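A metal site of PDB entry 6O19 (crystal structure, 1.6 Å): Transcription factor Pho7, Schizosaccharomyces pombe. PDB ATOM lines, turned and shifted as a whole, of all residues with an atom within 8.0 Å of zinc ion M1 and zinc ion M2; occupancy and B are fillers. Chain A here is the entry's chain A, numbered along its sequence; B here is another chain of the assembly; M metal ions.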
ATOM      1  N   ALA A  11      -8.806   2.634 -16.214  1.00  0.00           N
ATOM      2  CA  ALA A  11      -9.373   2.669 -17.553  1.00  0.00           C
ATOM      3  C   ALA A  11      -8.417   3.397 -18.494  1.00  0.00           C
ATOM      4  O   ALA A  11      -7.689   4.311 -18.088  1.00  0.00           O
ATOM      5  CB  ALA A  11     -10.724   3.362 -17.538  1.00  0.00           C
ATOM      6  N   ARG A  13      -9.229   5.529 -20.684  1.00  0.00           N
ATOM      7  CA  ARG A  13      -9.677   6.891 -20.474  1.00  0.00           C
ATOM      8  C   ARG A  13     -11.059   6.852 -19.824  1.00  0.00           C
ATOM      9  O   ARG A  13     -11.797   5.880 -19.958  1.00  0.00           O
ATOM     10  CB  ARG A  13      -9.707   7.708 -21.787  1.00  0.00           C
ATOM     11  CG  ARG A  13     -10.945   7.475 -22.619  1.00  0.00           C
ATOM     12  CD  ARG A  13     -10.849   8.082 -24.028  1.00  0.00           C
ATOM     13  NE  ARG A  13     -10.204   9.400 -24.094  1.00  0.00           N
ATOM     14  CZ  ARG A  13     -10.801  10.552 -23.752  1.00  0.00           C
ATOM     15  NH1 ARG A  13     -12.036  10.561 -23.269  1.00  0.00           N
ATOM     16  NH2 ARG A  13     -10.141  11.692 -23.885  1.00  0.00           N
ATOM     17  N   ALA A  14     -11.380   7.919 -19.107  1.00  0.00           N
ATOM     18  CA  ALA A  14     -12.661   8.010 -18.414  1.00  0.00           C
ATOM     19  C   ALA A  14     -13.644   8.837 -19.230  1.00  0.00           C
ATOM     20  O   ALA A  14     -13.278   9.842 -19.837  1.00  0.00           O
ATOM     21  CB  ALA A  14     -12.482   8.616 -17.023  1.00  0.00           C
ATOM     22  N   CYS A  15     -14.890   8.389 -19.255  1.00  0.00           N
ATOM     23  CA  CYS A  15     -15.956   9.121 -19.916  1.00  0.00           C
ATOM     24  C   CYS A  15     -16.340  10.355 -19.088  1.00  0.00           C
ATOM     25  O   CYS A  15     -15.975  10.500 -17.921  1.00  0.00           O
ATOM     26  CB  CYS A  15     -17.179   8.222 -20.107  1.00  0.00           C
ATOM     27  SG  CYS A  15     -18.086   7.879 -18.533  1.00  0.00           S
ATOM     28  N   ALA A  16     -17.154  11.212 -19.703  1.00  0.00           N
ATOM     29  CA  ALA A  16     -17.442  12.500 -19.094  1.00  0.00           C
ATOM     30  C   ALA A  16     -18.139  12.351 -17.741  1.00  0.00           C
ATOM     31  O   ALA A  16     -17.853  13.121 -16.819  1.00  0.00           O
ATOM     32  CB  ALA A  16     -18.273  13.364 -20.046  1.00  0.00           C
ATOM     33  N   LYS A  17     -19.051  11.386 -17.602  1.00  0.00           N
ATOM     34  CA  LYS A  17     -19.752  11.255 -16.330  1.00  0.00           C
ATOM     35  C   LYS A  17     -18.837  10.717 -15.235  1.00  0.00           C
ATOM     36  O   LYS A  17     -18.852  11.218 -14.104  1.00  0.00           O
ATOM     37  CB  LYS A  17     -20.995  10.390 -16.455  1.00  0.00           C
ATOM     38  CG  LYS A  17     -21.691  10.202 -15.118  1.00  0.00           C
ATOM     39  CD  LYS A  17     -22.934   9.372 -15.255  1.00  0.00           C
ATOM     40  CE  LYS A  17     -23.304   8.698 -13.943  1.00  0.00           C
ATOM     41  NZ  LYS A  17     -23.608   9.699 -12.874  1.00  0.00           N
ATOM     42  N   CYS A  18     -18.006   9.712 -15.548  1.00  0.00           N
ATOM     43  CA  CYS A  18     -17.050   9.231 -14.553  1.00  0.00           C
ATOM     44  C   CYS A  18     -16.053  10.320 -14.186  1.00  0.00           C
ATOM     45  O   CYS A  18     -15.623  10.407 -13.024  1.00  0.00           O
ATOM     46  CB  CYS A  18     -16.332   7.986 -15.072  1.00  0.00           C
ATOM     47  SG  CYS A  18     -17.400   6.512 -15.081  1.00  0.00           S
ATOM     48  N   GLN A  19     -15.670  11.162 -15.142  1.00  0.00           N
ATOM     49  CA  GLN A  19     -14.817  12.308 -14.829  1.00  0.00           C
ATOM     50  C   GLN A  19     -15.517  13.264 -13.863  1.00  0.00           C
ATOM     51  O   GLN A  19     -14.933  13.678 -12.856  1.00  0.00           O
ATOM     52  CB  GLN A  19     -14.414  13.036 -16.104  1.00  0.00           C
ATOM     53  CG  GLN A  19     -13.418  12.267 -16.967  1.00  0.00           C
ATOM     54  CD  GLN A  19     -13.220  12.881 -18.332  1.00  0.00           C
ATOM     55  OE1 GLN A  19     -14.167  13.378 -18.951  1.00  0.00           O
ATOM     56  NE2 GLN A  19     -11.990  12.853 -18.806  1.00  0.00           N
ATOM     57  N   LYS A  23     -15.253   8.941 -10.379  1.00  0.00           N
ATOM     58  CA  LYS A  23     -15.479   7.529 -10.112  1.00  0.00           C
ATOM     59  C   LYS A  23     -14.801   6.661 -11.184  1.00  0.00           C
ATOM     60  O   LYS A  23     -14.267   7.162 -12.175  1.00  0.00           O
ATOM     61  CB  LYS A  23     -16.984   7.238 -10.016  1.00  0.00           C
ATOM     62  CG  LYS A  23     -17.655   7.816  -8.776  1.00  0.00           C
ATOM     63  CD  LYS A  23     -17.089   7.199  -7.507  1.00  0.00           C
ATOM     64  CE  LYS A  23     -17.935   7.529  -6.287  1.00  0.00           C
ATOM     65  NZ  LYS A  23     -17.245   7.066  -5.037  1.00  0.00           N
ATOM     66  N   LYS A  24     -14.848   5.350 -10.969  1.00  0.00           N
ATOM     67  CA  LYS A  24     -14.082   4.383 -11.754  1.00  0.00           C
ATOM     68  C   LYS A  24     -14.771   4.113 -13.082  1.00  0.00           C
ATOM     69  O   LYS A  24     -15.871   3.552 -13.103  1.00  0.00           O
ATOM     70  CB  LYS A  24     -13.924   3.100 -10.939  1.00  0.00           C
ATOM     71  CG  LYS A  24     -13.186   1.966 -11.636  1.00  0.00           C
ATOM     72  CD  LYS A  24     -11.690   2.176 -11.537  1.00  0.00           C
ATOM     73  CE  LYS A  24     -10.923   1.112 -12.308  1.00  0.00           C
ATOM     74  NZ  LYS A  24     -11.000   1.392 -13.769  1.00  0.00           N
ATOM     75  N   CYS A  25     -14.130   4.477 -14.181  1.00  0.00           N
ATOM     76  CA  CYS A  25     -14.638   4.154 -15.519  1.00  0.00           C
ATOM     77  C   CYS A  25     -14.117   2.766 -15.923  1.00  0.00           C
ATOM     78  O   CYS A  25     -13.557   2.025 -15.102  1.00  0.00           O
ATOM     79  CB  CYS A  25     -14.259   5.250 -16.517  1.00  0.00           C
ATOM     80  SG  CYS A  25     -15.236   5.252 -18.062  1.00  0.00           S
ATOM     81  N   ASP A  26     -14.320   2.377 -17.174  1.00  0.00           N
ATOM     82  CA  ASP A  26     -13.764   1.135 -17.690  1.00  0.00           C
ATOM     83  C   ASP A  26     -13.566   1.293 -19.192  1.00  0.00           C
ATOM     84  O   ASP A  26     -13.648   2.410 -19.726  1.00  0.00           O
ATOM     85  CB  ASP A  26     -14.631  -0.076 -17.302  1.00  0.00           C
ATOM     86  CG  ASP A  26     -16.085   0.071 -17.749  1.00  0.00           C
ATOM     87  OD1 ASP A  26     -16.335   0.037 -18.957  1.00  0.00           O
ATOM     88  OD2 ASP A  26     -16.972   0.204 -16.875  1.00  0.00           O
ATOM     89  N   ASP A  27     -13.263   0.193 -19.884  1.00  0.00           N
ATOM     90  CA  ASP A  27     -12.945   0.290 -21.303  1.00  0.00           C
ATOM     91  C   ASP A  27     -14.120  -0.092 -22.200  1.00  0.00           C
ATOM     92  O   ASP A  27     -13.961  -0.082 -23.432  1.00  0.00           O
ATOM     93  CB  ASP A  27     -11.723  -0.569 -21.613  1.00  0.00           C
ATOM     94  CG  ASP A  27     -10.494  -0.128 -20.823  1.00  0.00           C
ATOM     95  OD1 ASP A  27     -10.309   1.109 -20.660  1.00  0.00           O
ATOM     96  OD2 ASP A  27      -9.722  -0.983 -20.345  1.00  0.00           O
ATOM     97  N   ALA A  28     -15.278  -0.394 -21.622  1.00  0.00           N
ATOM     98  CA  ALA A  28     -16.494  -0.562 -22.406  1.00  0.00           C
ATOM     99  C   ALA A  28     -17.080   0.805 -22.743  1.00  0.00           C
ATOM    100  O   ALA A  28     -16.944   1.768 -21.987  1.00  0.00           O
ATOM    101  CB  ALA A  28     -17.526  -1.366 -21.620  1.00  0.00           C
ATOM    102  N   ARG A  29     -17.767   0.874 -23.890  1.00  0.00           N
ATOM    103  CA  ARG A  29     -18.511   2.080 -24.251  1.00  0.00           C
ATOM    104  C   ARG A  29     -19.873   1.674 -24.799  1.00  0.00           C
ATOM    105  O   ARG A  29     -19.956   1.099 -25.886  1.00  0.00           O
ATOM    106  CB  ARG A  29     -17.746   2.931 -25.264  1.00  0.00           C
ATOM    107  CG  ARG A  29     -16.529   3.638 -24.675  1.00  0.00           C
ATOM    108  CD  ARG A  29     -16.942   4.649 -23.638  1.00  0.00           C
ATOM    109  NE  ARG A  29     -15.816   5.467 -23.160  1.00  0.00           N
ATOM    110  CZ  ARG A  29     -15.079   5.183 -22.082  1.00  0.00           C
ATOM    111  NH1 ARG A  29     -15.337   4.093 -21.353  1.00  0.00           N
ATOM    112  NH2 ARG A  29     -14.088   5.995 -21.727  1.00  0.00           N
ATOM    113  N   PRO A  30     -20.979   1.953 -24.071  1.00  0.00           N
ATOM    114  CA  PRO A  30     -21.001   2.696 -22.803  1.00  0.00           C
ATOM    115  C   PRO A  30     -20.334   1.971 -21.638  1.00  0.00           C
ATOM    116  O   PRO A  30     -20.332   0.738 -21.612  1.00  0.00           O
ATOM    117  CB  PRO A  30     -22.506   2.865 -22.541  1.00  0.00           C
ATOM    118  CG  PRO A  30     -23.152   1.684 -23.279  1.00  0.00           C
ATOM    119  CD  PRO A  30     -22.321   1.545 -24.518  1.00  0.00           C
ATOM    120  N   CYS A  31     -19.771   2.733 -20.701  1.00  0.00           N
ATOM    121  CA  CYS A  31     -19.116   2.126 -19.546  1.00  0.00           C
ATOM    122  C   CYS A  31     -20.157   1.582 -18.575  1.00  0.00           C
ATOM    123  O   CYS A  31     -21.344   1.906 -18.655  1.00  0.00           O
ATOM    124  CB  CYS A  31     -18.206   3.154 -18.866  1.00  0.00           C
ATOM    125  SG  CYS A  31     -19.073   4.421 -17.903  1.00  0.00           S
ATOM    126  N   GLN A  32     -19.708   0.748 -17.643  1.00  0.00           N
ATOM    127  CA  GLN A  32     -20.669   0.064 -16.773  1.00  0.00           C
ATOM    128  C   GLN A  32     -21.425   1.061 -15.892  1.00  0.00           C
ATOM    129  O   GLN A  32     -22.624   0.894 -15.648  1.00  0.00           O
ATOM    130  CB  GLN A  32     -19.972  -0.990 -15.926  1.00  0.00           C
ATOM    131  CG  GLN A  32     -19.329  -2.098 -16.765  1.00  0.00           C
ATOM    132  CD  GLN A  32     -20.268  -2.616 -17.837  1.00  0.00           C
ATOM    133  OE1 GLN A  32     -21.305  -3.205 -17.524  1.00  0.00           O
ATOM    134  NE2 GLN A  32     -19.921  -2.398 -19.101  1.00  0.00           N
ATOM    135  N   ARG A  33     -20.753   2.118 -15.429  1.00  0.00           N
ATOM    136  CA  ARG A  33     -21.440   3.078 -14.563  1.00  0.00           C
ATOM    137  C   ARG A  33     -22.533   3.817 -15.319  1.00  0.00           C
ATOM    138  O   ARG A  33     -23.578   4.146 -14.746  1.00  0.00           O
ATOM    139  CB  ARG A  33     -20.453   4.070 -13.940  1.00  0.00           C
ATOM    140  CG  ARG A  33     -19.649   3.534 -12.762  1.00  0.00           C
ATOM    141  CD  ARG A  33     -18.886   4.669 -12.036  1.00  0.00           C
ATOM    142  NE  ARG A  33     -19.749   5.481 -11.176  1.00  0.00           N
ATOM    143  CZ  ARG A  33     -20.093   6.743 -11.407  1.00  0.00           C
ATOM    144  NH1 ARG A  33     -19.641   7.374 -12.496  1.00  0.00           N
ATOM    145  NH2 ARG A  33     -20.878   7.389 -10.565  1.00  0.00           N
ATOM    146  N   CYS A  34     -22.301   4.112 -16.610  1.00  0.00           N
ATOM    147  CA  CYS A  34     -23.306   4.812 -17.394  1.00  0.00           C
ATOM    148  C   CYS A  34     -24.492   3.894 -17.725  1.00  0.00           C
ATOM    149  O   CYS A  34     -25.642   4.357 -17.751  1.00  0.00           O
ATOM    150  CB  CYS A  34     -22.681   5.373 -18.677  1.00  0.00           C
ATOM    151  SG  CYS A  34     -21.748   6.927 -18.368  1.00  0.00           S
ATOM    152  N   ILE A  35     -24.229   2.607 -17.963  1.00  0.00           N
ATOM    153  CA  ILE A  35     -25.342   1.675 -18.197  1.00  0.00           C
ATOM    154  C   ILE A  35     -26.251   1.632 -16.985  1.00  0.00           C
ATOM    155  O   ILE A  35     -27.481   1.762 -17.096  1.00  0.00           O
ATOM    156  CB  ILE A  35     -24.798   0.276 -18.556  1.00  0.00           C
ATOM    157  CG1 ILE A  35     -24.070   0.320 -19.894  1.00  0.00           C
ATOM    158  CG2 ILE A  35     -25.947  -0.734 -18.638  1.00  0.00           C
ATOM    159  CD1 ILE A  35     -23.327  -0.947 -20.245  1.00  0.00           C
ATOM    160  N   THR A  39     -27.238   6.962 -18.204  1.00  0.00           N
ATOM    161  CA  THR A  39     -26.731   8.261 -18.605  1.00  0.00           C
ATOM    162  C   THR A  39     -25.864   8.120 -19.858  1.00  0.00           C
ATOM    163  O   THR A  39     -25.129   7.153 -20.007  1.00  0.00           O
ATOM    164  CB  THR A  39     -25.881   8.893 -17.501  1.00  0.00           C
ATOM    165  OG1 THR A  39     -24.846   7.978 -17.122  1.00  0.00           O
ATOM    166  CG2 THR A  39     -26.738   9.231 -16.283  1.00  0.00           C
ATOM    167  N   ASP A  40     -25.970   9.114 -20.746  1.00  0.00           N
ATOM    168  CA  ASP A  40     -25.136   9.162 -21.940  1.00  0.00           C
ATOM    169  C   ASP A  40     -23.669   9.007 -21.583  1.00  0.00           C
ATOM    170  O   ASP A  40     -23.156   9.677 -20.685  1.00  0.00           O
ATOM    171  CB  ASP A  40     -25.396  10.504 -22.644  1.00  0.00           C
ATOM    172  CG  ASP A  40     -24.796  10.592 -24.041  1.00  0.00           C
ATOM    173  OD1 ASP A  40     -24.386   9.554 -24.617  1.00  0.00           O
ATOM    174  OD2 ASP A  40     -24.733  11.719 -24.572  1.00  0.00           O
ATOM    175  N   CYS A  41     -22.987   8.107 -22.293  1.00  0.00           N
ATOM    176  CA  CYS A  41     -21.567   7.848 -22.060  1.00  0.00           C
ATOM    177  C   CYS A  41     -20.778   8.458 -23.210  1.00  0.00           C
ATOM    178  O   CYS A  41     -20.745   7.910 -24.319  1.00  0.00           O
ATOM    179  CB  CYS A  41     -21.320   6.335 -21.932  1.00  0.00           C
ATOM    180  SG  CYS A  41     -19.620   5.920 -21.485  1.00  0.00           S
ATOM    181  N   ILE A  42     -20.137   9.598 -22.951  1.00  0.00           N
ATOM    182  CA  ILE A  42     -19.463  10.388 -23.986  1.00  0.00           C
ATOM    183  C   ILE A  42     -18.001  10.560 -23.589  1.00  0.00           C
ATOM    184  O   ILE A  42     -17.708  10.840 -22.421  1.00  0.00           O
ATOM    185  CB  ILE A  42     -20.093  11.781 -24.163  1.00  0.00           C
ATOM    186  CG1 ILE A  42     -21.608  11.731 -24.057  1.00  0.00           C
ATOM    187  CG2 ILE A  42     -19.659  12.408 -25.488  1.00  0.00           C
ATOM    188  CD1 ILE A  42     -22.199  13.049 -23.616  1.00  0.00           C
ATOM    189  N   ASP A  43     -17.101  10.454 -24.567  1.00  0.00           N
ATOM    190  CA  ASP A  43     -15.690  10.785 -24.357  1.00  0.00           C
ATOM    191  C   ASP A  43     -15.402  12.219 -24.804  1.00  0.00           C
ATOM    192  O   ASP A  43     -15.766  12.618 -25.917  1.00  0.00           O
ATOM    193  CB  ASP A  43     -14.792   9.804 -25.101  1.00  0.00           C
ATOM    194  CG  ASP A  43     -14.642   8.493 -24.368  1.00  0.00           C
ATOM    195  OD1 ASP A  43     -14.200   8.512 -23.189  1.00  0.00           O
ATOM    196  OD2 ASP A  43     -14.965   7.446 -24.967  1.00  0.00           O
ATOM    197  P    DC B  12     -10.295   5.325 -13.706  1.00  0.00           P
ATOM    198  OP1  DC B  12      -9.919   3.925 -14.033  1.00  0.00           O
ATOM    199  OP2  DC B  12     -11.507   5.942 -14.227  1.00  0.00           O
ATOM    200  O5'  DC B  12     -10.361   5.490 -12.110  1.00  0.00           O
ATOM    201  C5'  DC B  12      -9.297   5.008 -11.311  1.00  0.00           C
ATOM    202  C4'  DC B  12      -9.496   5.395  -9.856  1.00  0.00           C
ATOM    203  O4'  DC B  12      -9.314   6.827  -9.705  1.00  0.00           O
ATOM    204  C3'  DC B  12     -10.890   5.088  -9.261  1.00  0.00           C
ATOM    205  O3'  DC B  12     -10.706   4.732  -7.909  1.00  0.00           O
ATOM    206  C2'  DC B  12     -11.579   6.435  -9.348  1.00  0.00           C
ATOM    207  C1'  DC B  12     -10.412   7.325  -8.950  1.00  0.00           C
ATOM    208  N1   DC B  12     -10.556   8.772  -9.231  1.00  0.00           N
ATOM    209  C2   DC B  12     -10.001   9.670  -8.327  1.00  0.00           C
ATOM    210  O2   DC B  12      -9.462   9.237  -7.305  1.00  0.00           O
ATOM    211  N3   DC B  12     -10.098  11.004  -8.569  1.00  0.00           N
ATOM    212  C4   DC B  12     -10.675  11.440  -9.692  1.00  0.00           C
ATOM    213  N4   DC B  12     -10.721  12.767  -9.897  1.00  0.00           N
ATOM    214  C5   DC B  12     -11.229  10.521 -10.657  1.00  0.00           C
ATOM    215  C6   DC B  12     -11.139   9.207 -10.389  1.00  0.00           C
HETATM  216 ZN    ZN M   1     -17.284   5.896 -17.292  1.00  0.00          ZN
HETATM  217 ZN    ZN M   2     -19.727   6.341 -19.225  1.00  0.00          ZN
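Four residues have an atom within 4 Å of zinc ion M2: Cys 15, Cys 31, Cys 34 and Cys 41. The nearest printed residue that does not touch zinc ion M2 is Cys 18 (4.8 Å).
Zinc ion M2 is bound by SG of Cys 34 (2.3 Å), SG of Cys 41 (2.3 Å), SG of Cys 15 (2.4 Å) and SG of Cys 31 (2.4 Å). Zinc ion M2 has four donor atoms within binding distance.
The side-chain sulfur (SG) of Cys 15 sits close to the backbone NH (N) of Lys 17 (3.8 Å). SG of Cys 31 sits close to N of Arg 33, 3.8 Å away. The side-chain sulfur (SG) of Cys 25 lies close to the guanidinium group (NH1) of Arg 29. The backbone carbonyl oxygen of Cys 34 lies within hydrogen-bond range of the backbone NH of Thr 39 (3.1 Å). The backbone NH of Lys 23 sits at hydrogen-bond distance from the backbone carbonyl oxygen of Cys 18 (3.0 Å). OP2 of DC 12 of chain B is in hydrogen-bond range of the backbone NH (N) of Cys 25 (3.0 Å). SG of Cys 18 lies close to NH1 of Arg 33 (3.5 Å).
Zinc ion M1 is bound by SG of Cys 25 (2.3 Å), SG of Cys 18 (2.3 Å), SG of Cys 31 (2.4 Å) and SG of Cys 15 (2.5 Å). Zinc ion M1 has four donor atoms within binding distance.
The nearest printed residue that does not touch zinc ion M1 is Asp 26 (4.6 Å).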
